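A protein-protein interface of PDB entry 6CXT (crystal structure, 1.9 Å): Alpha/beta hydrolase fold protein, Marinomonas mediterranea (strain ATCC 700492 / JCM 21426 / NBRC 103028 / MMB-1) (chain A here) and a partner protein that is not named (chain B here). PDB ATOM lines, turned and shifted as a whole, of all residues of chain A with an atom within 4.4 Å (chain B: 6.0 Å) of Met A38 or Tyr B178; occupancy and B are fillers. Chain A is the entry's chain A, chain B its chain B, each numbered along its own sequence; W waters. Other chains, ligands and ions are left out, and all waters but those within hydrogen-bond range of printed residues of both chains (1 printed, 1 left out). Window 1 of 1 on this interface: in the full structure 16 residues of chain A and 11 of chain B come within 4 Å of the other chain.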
ATOM      1  N   LEU A  33       3.326  -3.227   4.505  1.00  0.00           N
ATOM      2  CA  LEU A  33       4.639  -2.741   4.864  1.00  0.00           C
ATOM      3  C   LEU A  33       5.614  -3.208   3.798  1.00  0.00           C
ATOM      4  O   LEU A  33       5.738  -4.407   3.532  1.00  0.00           O
ATOM      5  CB  LEU A  33       5.142  -3.263   6.204  1.00  0.00           C
ATOM      6  CG  LEU A  33       4.514  -2.750   7.473  1.00  0.00           C
ATOM      7  CD1 LEU A  33       5.430  -3.141   8.629  1.00  0.00           C
ATOM      8  CD2 LEU A  33       4.324  -1.243   7.416  1.00  0.00           C
ATOM      9  N   ASP A  34       6.246  -2.264   3.134  1.00  0.00           N
ATOM     10  CA  ASP A  34       7.219  -2.544   2.089  1.00  0.00           C
ATOM     11  C   ASP A  34       8.401  -1.582   2.219  1.00  0.00           C
ATOM     12  O   ASP A  34       8.456  -0.844   3.146  1.00  0.00           O
ATOM     13  CB  ASP A  34       6.581  -2.538   0.701  1.00  0.00           C
ATOM     14  CG  ASP A  34       6.017  -1.164   0.286  1.00  0.00           C
ATOM     15  OD1 ASP A  34       6.469  -0.130   0.752  1.00  0.00           O
ATOM     16  OD2 ASP A  34       5.106  -1.143  -0.516  1.00  0.00           O
ATOM     17  N   SER A  35       9.325  -1.595   1.273  1.00  0.00           N
ATOM     18  CA  SER A  35      10.505  -0.767   1.422  1.00  0.00           C
ATOM     19  C   SER A  35      10.169   0.743   1.618  1.00  0.00           C
ATOM     20  O   SER A  35      10.844   1.425   2.378  1.00  0.00           O
ATOM     21  CB  SER A  35      11.316  -0.887   0.118  1.00  0.00           C
ATOM     22  OG  SER A  35      12.288   0.137   0.123  1.00  0.00           O
ATOM     23  N   LEU A  36       9.159   1.227   0.900  1.00  0.00           N
ATOM     24  CA  LEU A  36       8.767   2.663   0.982  1.00  0.00           C
ATOM     25  C   LEU A  36       7.927   2.925   2.276  1.00  0.00           C
ATOM     26  O   LEU A  36       8.278   3.833   3.037  1.00  0.00           O
ATOM     27  CB  LEU A  36       7.991   3.068  -0.262  1.00  0.00           C
ATOM     28  CG  LEU A  36       8.883   2.978  -1.550  1.00  0.00           C
ATOM     29  CD1 LEU A  36       8.102   3.510  -2.715  1.00  0.00           C
ATOM     30  CD2 LEU A  36      10.212   3.730  -1.482  1.00  0.00           C
ATOM     31  N   SER A  37       6.862   2.136   2.489  1.00  0.00           N
ATOM     32  CA  SER A  37       5.999   2.399   3.671  1.00  0.00           C
ATOM     33  C   SER A  37       6.767   2.198   4.959  1.00  0.00           C
ATOM     34  O   SER A  37       6.467   2.886   5.945  1.00  0.00           O
ATOM     35  CB  SER A  37       4.712   1.619   3.634  1.00  0.00           C
ATOM     36  OG  SER A  37       5.001   0.225   3.538  1.00  0.00           O
ATOM     37  N   MET A  38       7.795   1.348   4.947  1.00  0.00           N
ATOM     38  CA  MET A  38       8.611   1.121   6.145  1.00  0.00           C
ATOM     39  C   MET A  38       9.313   2.397   6.559  1.00  0.00           C
ATOM     40  O   MET A  38       9.347   2.747   7.728  1.00  0.00           O
ATOM     41  CB  MET A  38       9.588  -0.051   5.929  1.00  0.00           C
ATOM     42  CG  MET A  38      10.546  -0.350   7.073  1.00  0.00           C
ATOM     43  SD  MET A  38       9.621  -1.032   8.506  1.00  0.00           S
ATOM     44  CE  MET A  38       8.944  -2.578   7.874  1.00  0.00           C
ATOM     45  N   VAL A  39       9.829   3.147   5.578  1.00  0.00           N
ATOM     46  CA  VAL A  39      10.520   4.396   5.874  1.00  0.00           C
ATOM     47  C   VAL A  39       9.570   5.364   6.582  1.00  0.00           C
ATOM     48  O   VAL A  39       9.957   6.013   7.548  1.00  0.00           O
ATOM     49  CB  VAL A  39      11.159   5.032   4.582  1.00  0.00           C
ATOM     50  CG1 VAL A  39      11.896   6.345   4.941  1.00  0.00           C
ATOM     51  CG2 VAL A  39      12.172   4.043   4.009  1.00  0.00           C
ATOM     52  N   LEU A  40       8.358   5.471   6.079  1.00  0.00           N
ATOM     53  CA  LEU A  40       7.400   6.437   6.643  1.00  0.00           C
ATOM     54  C   LEU A  40       6.999   5.955   8.086  1.00  0.00           C
ATOM     55  O   LEU A  40       6.885   6.749   9.037  1.00  0.00           O
ATOM     56  CB  LEU A  40       6.156   6.532   5.738  1.00  0.00           C
ATOM     57  CG  LEU A  40       6.448   7.090   4.296  1.00  0.00           C
ATOM     58  CD1 LEU A  40       5.160   7.209   3.521  1.00  0.00           C
ATOM     59  CD2 LEU A  40       7.164   8.418   4.379  1.00  0.00           C
ATOM     60  N   LEU A  41       6.773   4.647   8.205  1.00  0.00           N
ATOM     61  CA  LEU A  41       6.400   4.072   9.515  1.00  0.00           C
ATOM     62  C   LEU A  41       7.540   4.321  10.522  1.00  0.00           C
ATOM     63  O   LEU A  41       7.302   4.837  11.616  1.00  0.00           O
ATOM     64  CB  LEU A  41       6.127   2.573   9.355  1.00  0.00           C
ATOM     65  CG  LEU A  41       5.707   1.819  10.661  1.00  0.00           C
ATOM     66  CD1 LEU A  41       4.376   2.333  11.215  1.00  0.00           C
ATOM     67  CD2 LEU A  41       5.604   0.331  10.354  1.00  0.00           C
ATOM     68  N   LEU A  42       8.779   3.994  10.149  1.00  0.00           N
ATOM     69  CA  LEU A  42       9.885   4.209  11.056  1.00  0.00           C
ATOM     70  C   LEU A  42      10.021   5.659  11.457  1.00  0.00           C
ATOM     71  O   LEU A  42      10.414   5.925  12.590  1.00  0.00           O
ATOM     72  CB  LEU A  42      11.235   3.675  10.543  1.00  0.00           C
ATOM     73  CG  LEU A  42      11.345   2.169  10.298  1.00  0.00           C
ATOM     74  CD1 LEU A  42      12.745   1.792   9.837  1.00  0.00           C
ATOM     75  CD2 LEU A  42      10.955   1.378  11.555  1.00  0.00           C
ATOM     76  N   PHE A  63       7.092  -7.276  12.931  1.00  0.00           N
ATOM     77  CA  PHE A  63       6.310  -6.482  11.962  1.00  0.00           C
ATOM     78  C   PHE A  63       5.180  -7.272  11.403  1.00  0.00           C
ATOM     79  O   PHE A  63       4.498  -6.871  10.437  1.00  0.00           O
ATOM     80  CB  PHE A  63       7.204  -5.855  10.888  1.00  0.00           C
ATOM     81  CG  PHE A  63       8.045  -4.735  11.420  1.00  0.00           C
ATOM     82  CD1 PHE A  63       9.226  -4.988  12.149  1.00  0.00           C
ATOM     83  CD2 PHE A  63       7.622  -3.401  11.258  1.00  0.00           C
ATOM     84  CE1 PHE A  63       9.992  -3.927  12.680  1.00  0.00           C
ATOM     85  CE2 PHE A  63       8.370  -2.358  11.792  1.00  0.00           C
ATOM     86  CZ  PHE A  63       9.563  -2.608  12.480  1.00  0.00           C
ATOM     87  N   SER B 135       9.666  -6.910  -5.136  1.00  0.00           N
ATOM     88  CA  SER B 135       8.920  -7.308  -3.928  1.00  0.00           C
ATOM     89  C   SER B 135       8.543  -8.781  -4.017  1.00  0.00           C
ATOM     90  O   SER B 135       8.298  -9.441  -3.001  1.00  0.00           O
ATOM     91  CB  SER B 135       7.627  -6.475  -3.768  1.00  0.00           C
ATOM     92  OG  SER B 135       6.659  -6.849  -4.768  1.00  0.00           O
ATOM     93  N   HIS B 176       6.257 -13.670   4.622  1.00  0.00           N
ATOM     94  CA  HIS B 176       6.889 -12.537   5.256  1.00  0.00           C
ATOM     95  C   HIS B 176       7.101 -11.284   4.291  1.00  0.00           C
ATOM     96  O   HIS B 176       7.708 -10.308   4.703  1.00  0.00           O
ATOM     97  CB  HIS B 176       8.153 -12.926   5.995  1.00  0.00           C
ATOM     98  CG  HIS B 176       7.923 -13.913   7.110  1.00  0.00           C
ATOM     99  ND1 HIS B 176       8.945 -14.643   7.690  1.00  0.00           N
ATOM    100  CD2 HIS B 176       6.782 -14.280   7.758  1.00  0.00           C
ATOM    101  CE1 HIS B 176       8.447 -15.407   8.651  1.00  0.00           C
ATOM    102  NE2 HIS B 176       7.137 -15.212   8.707  1.00  0.00           N
ATOM    103  N   GLY B 177       6.559 -11.358   3.070  1.00  0.00           N
ATOM    104  CA  GLY B 177       6.622 -10.281   2.010  1.00  0.00           C
ATOM    105  C   GLY B 177       8.011  -9.683   1.916  1.00  0.00           C
ATOM    106  O   GLY B 177       9.008 -10.396   1.681  1.00  0.00           O
ATOM    107  N   TYR B 178       8.069  -8.375   2.194  1.00  0.00           N
ATOM    108  CA  TYR B 178       9.281  -7.559   2.206  1.00  0.00           C
ATOM    109  C   TYR B 178      10.389  -8.101   3.076  1.00  0.00           C
ATOM    110  O   TYR B 178      11.585  -7.905   2.776  1.00  0.00           O
ATOM    111  CB  TYR B 178       8.874  -6.100   2.628  1.00  0.00           C
ATOM    112  CG  TYR B 178       9.959  -5.131   3.010  1.00  0.00           C
ATOM    113  CD1 TYR B 178      10.960  -4.762   2.095  1.00  0.00           C
ATOM    114  CD2 TYR B 178       9.969  -4.538   4.292  1.00  0.00           C
ATOM    115  CE1 TYR B 178      11.952  -3.842   2.453  1.00  0.00           C
ATOM    116  CE2 TYR B 178      10.952  -3.621   4.670  1.00  0.00           C
ATOM    117  CZ  TYR B 178      11.943  -3.269   3.738  1.00  0.00           C
ATOM    118  OH  TYR B 178      12.905  -2.350   4.102  1.00  0.00           O
ATOM    119  N   LEU B 179      10.029  -8.792   4.169  1.00  0.00           N
ATOM    120  CA  LEU B 179      11.070  -9.321   5.042  1.00  0.00           C
ATOM    121  C   LEU B 179      11.173 -10.861   4.876  1.00  0.00           C
ATOM    122  O   LEU B 179      11.622 -11.582   5.793  1.00  0.00           O
ATOM    123  CB  LEU B 179      10.854  -8.879   6.491  1.00  0.00           C
ATOM    124  CG  LEU B 179      10.792  -7.361   6.718  1.00  0.00           C
ATOM    125  CD1 LEU B 179      10.335  -7.112   8.150  1.00  0.00           C
ATOM    126  CD2 LEU B 179      12.163  -6.684   6.493  1.00  0.00           C
ATOM    127  N   GLY B 180      10.729 -11.330   3.710  1.00  0.00           N
ATOM    128  CA  GLY B 180      10.804 -12.755   3.344  1.00  0.00           C
ATOM    129  C   GLY B 180      11.808 -13.209   2.274  1.00  0.00           C
ATOM    130  O   GLY B 180      11.625 -14.299   1.666  1.00  0.00           O
ATOM    131  N   GLN B 181      12.887 -12.435   2.090  1.00  0.00           N
ATOM    132  CA  GLN B 181      13.885 -12.752   1.080  1.00  0.00           C
ATOM    133  C   GLN B 181      15.196 -12.898   1.767  1.00  0.00           C
ATOM    134  O   GLN B 181      15.380 -12.377   2.849  1.00  0.00           O
ATOM    135  CB  GLN B 181      13.960 -11.595   0.005  1.00  0.00           C
ATOM    136  CG  GLN B 181      12.718 -11.489  -0.834  1.00  0.00           C
ATOM    137  CD  GLN B 181      12.654 -10.191  -1.672  1.00  0.00           C
ATOM    138  OE1 GLN B 181      13.504  -9.331  -1.527  1.00  0.00           O
ATOM    139  NE2 GLN B 181      11.654 -10.080  -2.536  1.00  0.00           N
ATOM    140  N   GLY B 229      15.573 -13.699   5.712  1.00  0.00           N
ATOM    141  CA  GLY B 229      14.619 -12.572   5.686  1.00  0.00           C
ATOM    142  C   GLY B 229      15.197 -11.171   5.464  1.00  0.00           C
ATOM    143  O   GLY B 229      14.416 -10.228   5.179  1.00  0.00           O
ATOM    144  N   GLY B 231      17.122 -10.163   3.072  1.00  0.00           N
ATOM    145  CA  GLY B 231      17.481 -10.035   1.646  1.00  0.00           C
ATOM    146  C   GLY B 231      17.125  -8.658   1.079  1.00  0.00           C
ATOM    147  O   GLY B 231      17.993  -8.003   0.455  1.00  0.00           O
ATOM    148  N   ALA B 232      15.874  -8.225   1.273  1.00  0.00           N
ATOM    149  CA  ALA B 232      15.446  -6.919   0.748  1.00  0.00           C
ATOM    150  C   ALA B 232      16.298  -5.751   1.253  1.00  0.00           C
ATOM    151  O   ALA B 232      16.679  -4.867   0.465  1.00  0.00           O
ATOM    152  CB  ALA B 232      13.975  -6.675   1.004  1.00  0.00           C
ATOM    153  N   ARG B 233      16.621  -5.741   2.542  1.00  0.00           N
ATOM    154  CA  ARG B 233      17.408  -4.669   3.146  1.00  0.00           C
ATOM    155  C   ARG B 233      18.886  -4.728   2.838  1.00  0.00           C
ATOM    156  O   ARG B 233      19.558  -3.690   2.714  1.00  0.00           O
ATOM    157  CB  ARG B 233      17.110  -4.527   4.656  1.00  0.00           C
ATOM    158  CG  ARG B 233      15.639  -4.141   4.883  1.00  0.00           C
ATOM    159  CD  ARG B 233      15.210  -4.035   6.350  1.00  0.00           C
ATOM    160  NE  ARG B 233      15.852  -2.912   7.016  1.00  0.00           N
ATOM    161  CZ  ARG B 233      15.427  -1.644   7.000  1.00  0.00           C
ATOM    162  NH1 ARG B 233      14.304  -1.269   6.362  1.00  0.00           N
ATOM    163  NH2 ARG B 233      16.142  -0.740   7.668  1.00  0.00           N
HETATM  164  O   HOH W   1       5.595  -6.998   2.705  1.00  0.00           O
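N of Leu A36 lies within hydrogen-bond range of OD1 of Asp A34.
The side-chain hydroxyl (OG) of Ser A37 sits at hydrogen-bond distance from the backbone NH (N) of Asp A34, 2.8 Å away.
The side-chain hydroxyl of Tyr B178 is in hydrogen-bond range of the guanidinium group of Arg B233, 2.9 Å away.
Among the printed residues, merely in contact across the chains: Leu A33 with Tyr B178 (3.7 Å), Asp A34 with Tyr B178 (3.9 Å), Ser A35 with Tyr B178 (3.6 Å), Met A38 with Tyr B178 (3.9 Å) and Met A38 with Arg B233 (3.9 Å).
Of chain B, only Tyr B178 (3.9 Å) and Arg B233 (3.9 Å) come within 4 Å of Met A38.
Printed residues of chain B within 4 Å of Asp A34: Tyr B178.
Printed residues of chain B within 4 Å of Ser A35: Tyr B178 (3.6 Å).
Printed residues of chain A within 4 Å of Arg B233: Met A38 (3.9 Å).
Of the printed residues of chain B, Leu A33 touches Tyr B178 (3.7 Å).
The nearest printed residue of chain A that does not touch Tyr B178 is Leu A36 (6.0 Å).
The nearest printed residue of chain B that does not touch Ser A35 is Arg B233 (5.9 Å).
Of the 11 printed residues of chain B, 2 touch a printed residue of chain A.
Hydrophobic or aromatic side chains of chain B that line the printed part of chain A: Tyr B178.
Among the printed residues, 5 pairs touch across the chains.
Among the printed residues, no Asp or Glu carboxylate lies within 4 Å of a Lys or Arg side-chain nitrogen of the other chain.
Water W1 bridges O of Leu A33 (2.7 Å) and N of Tyr B178 (2.9 Å).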
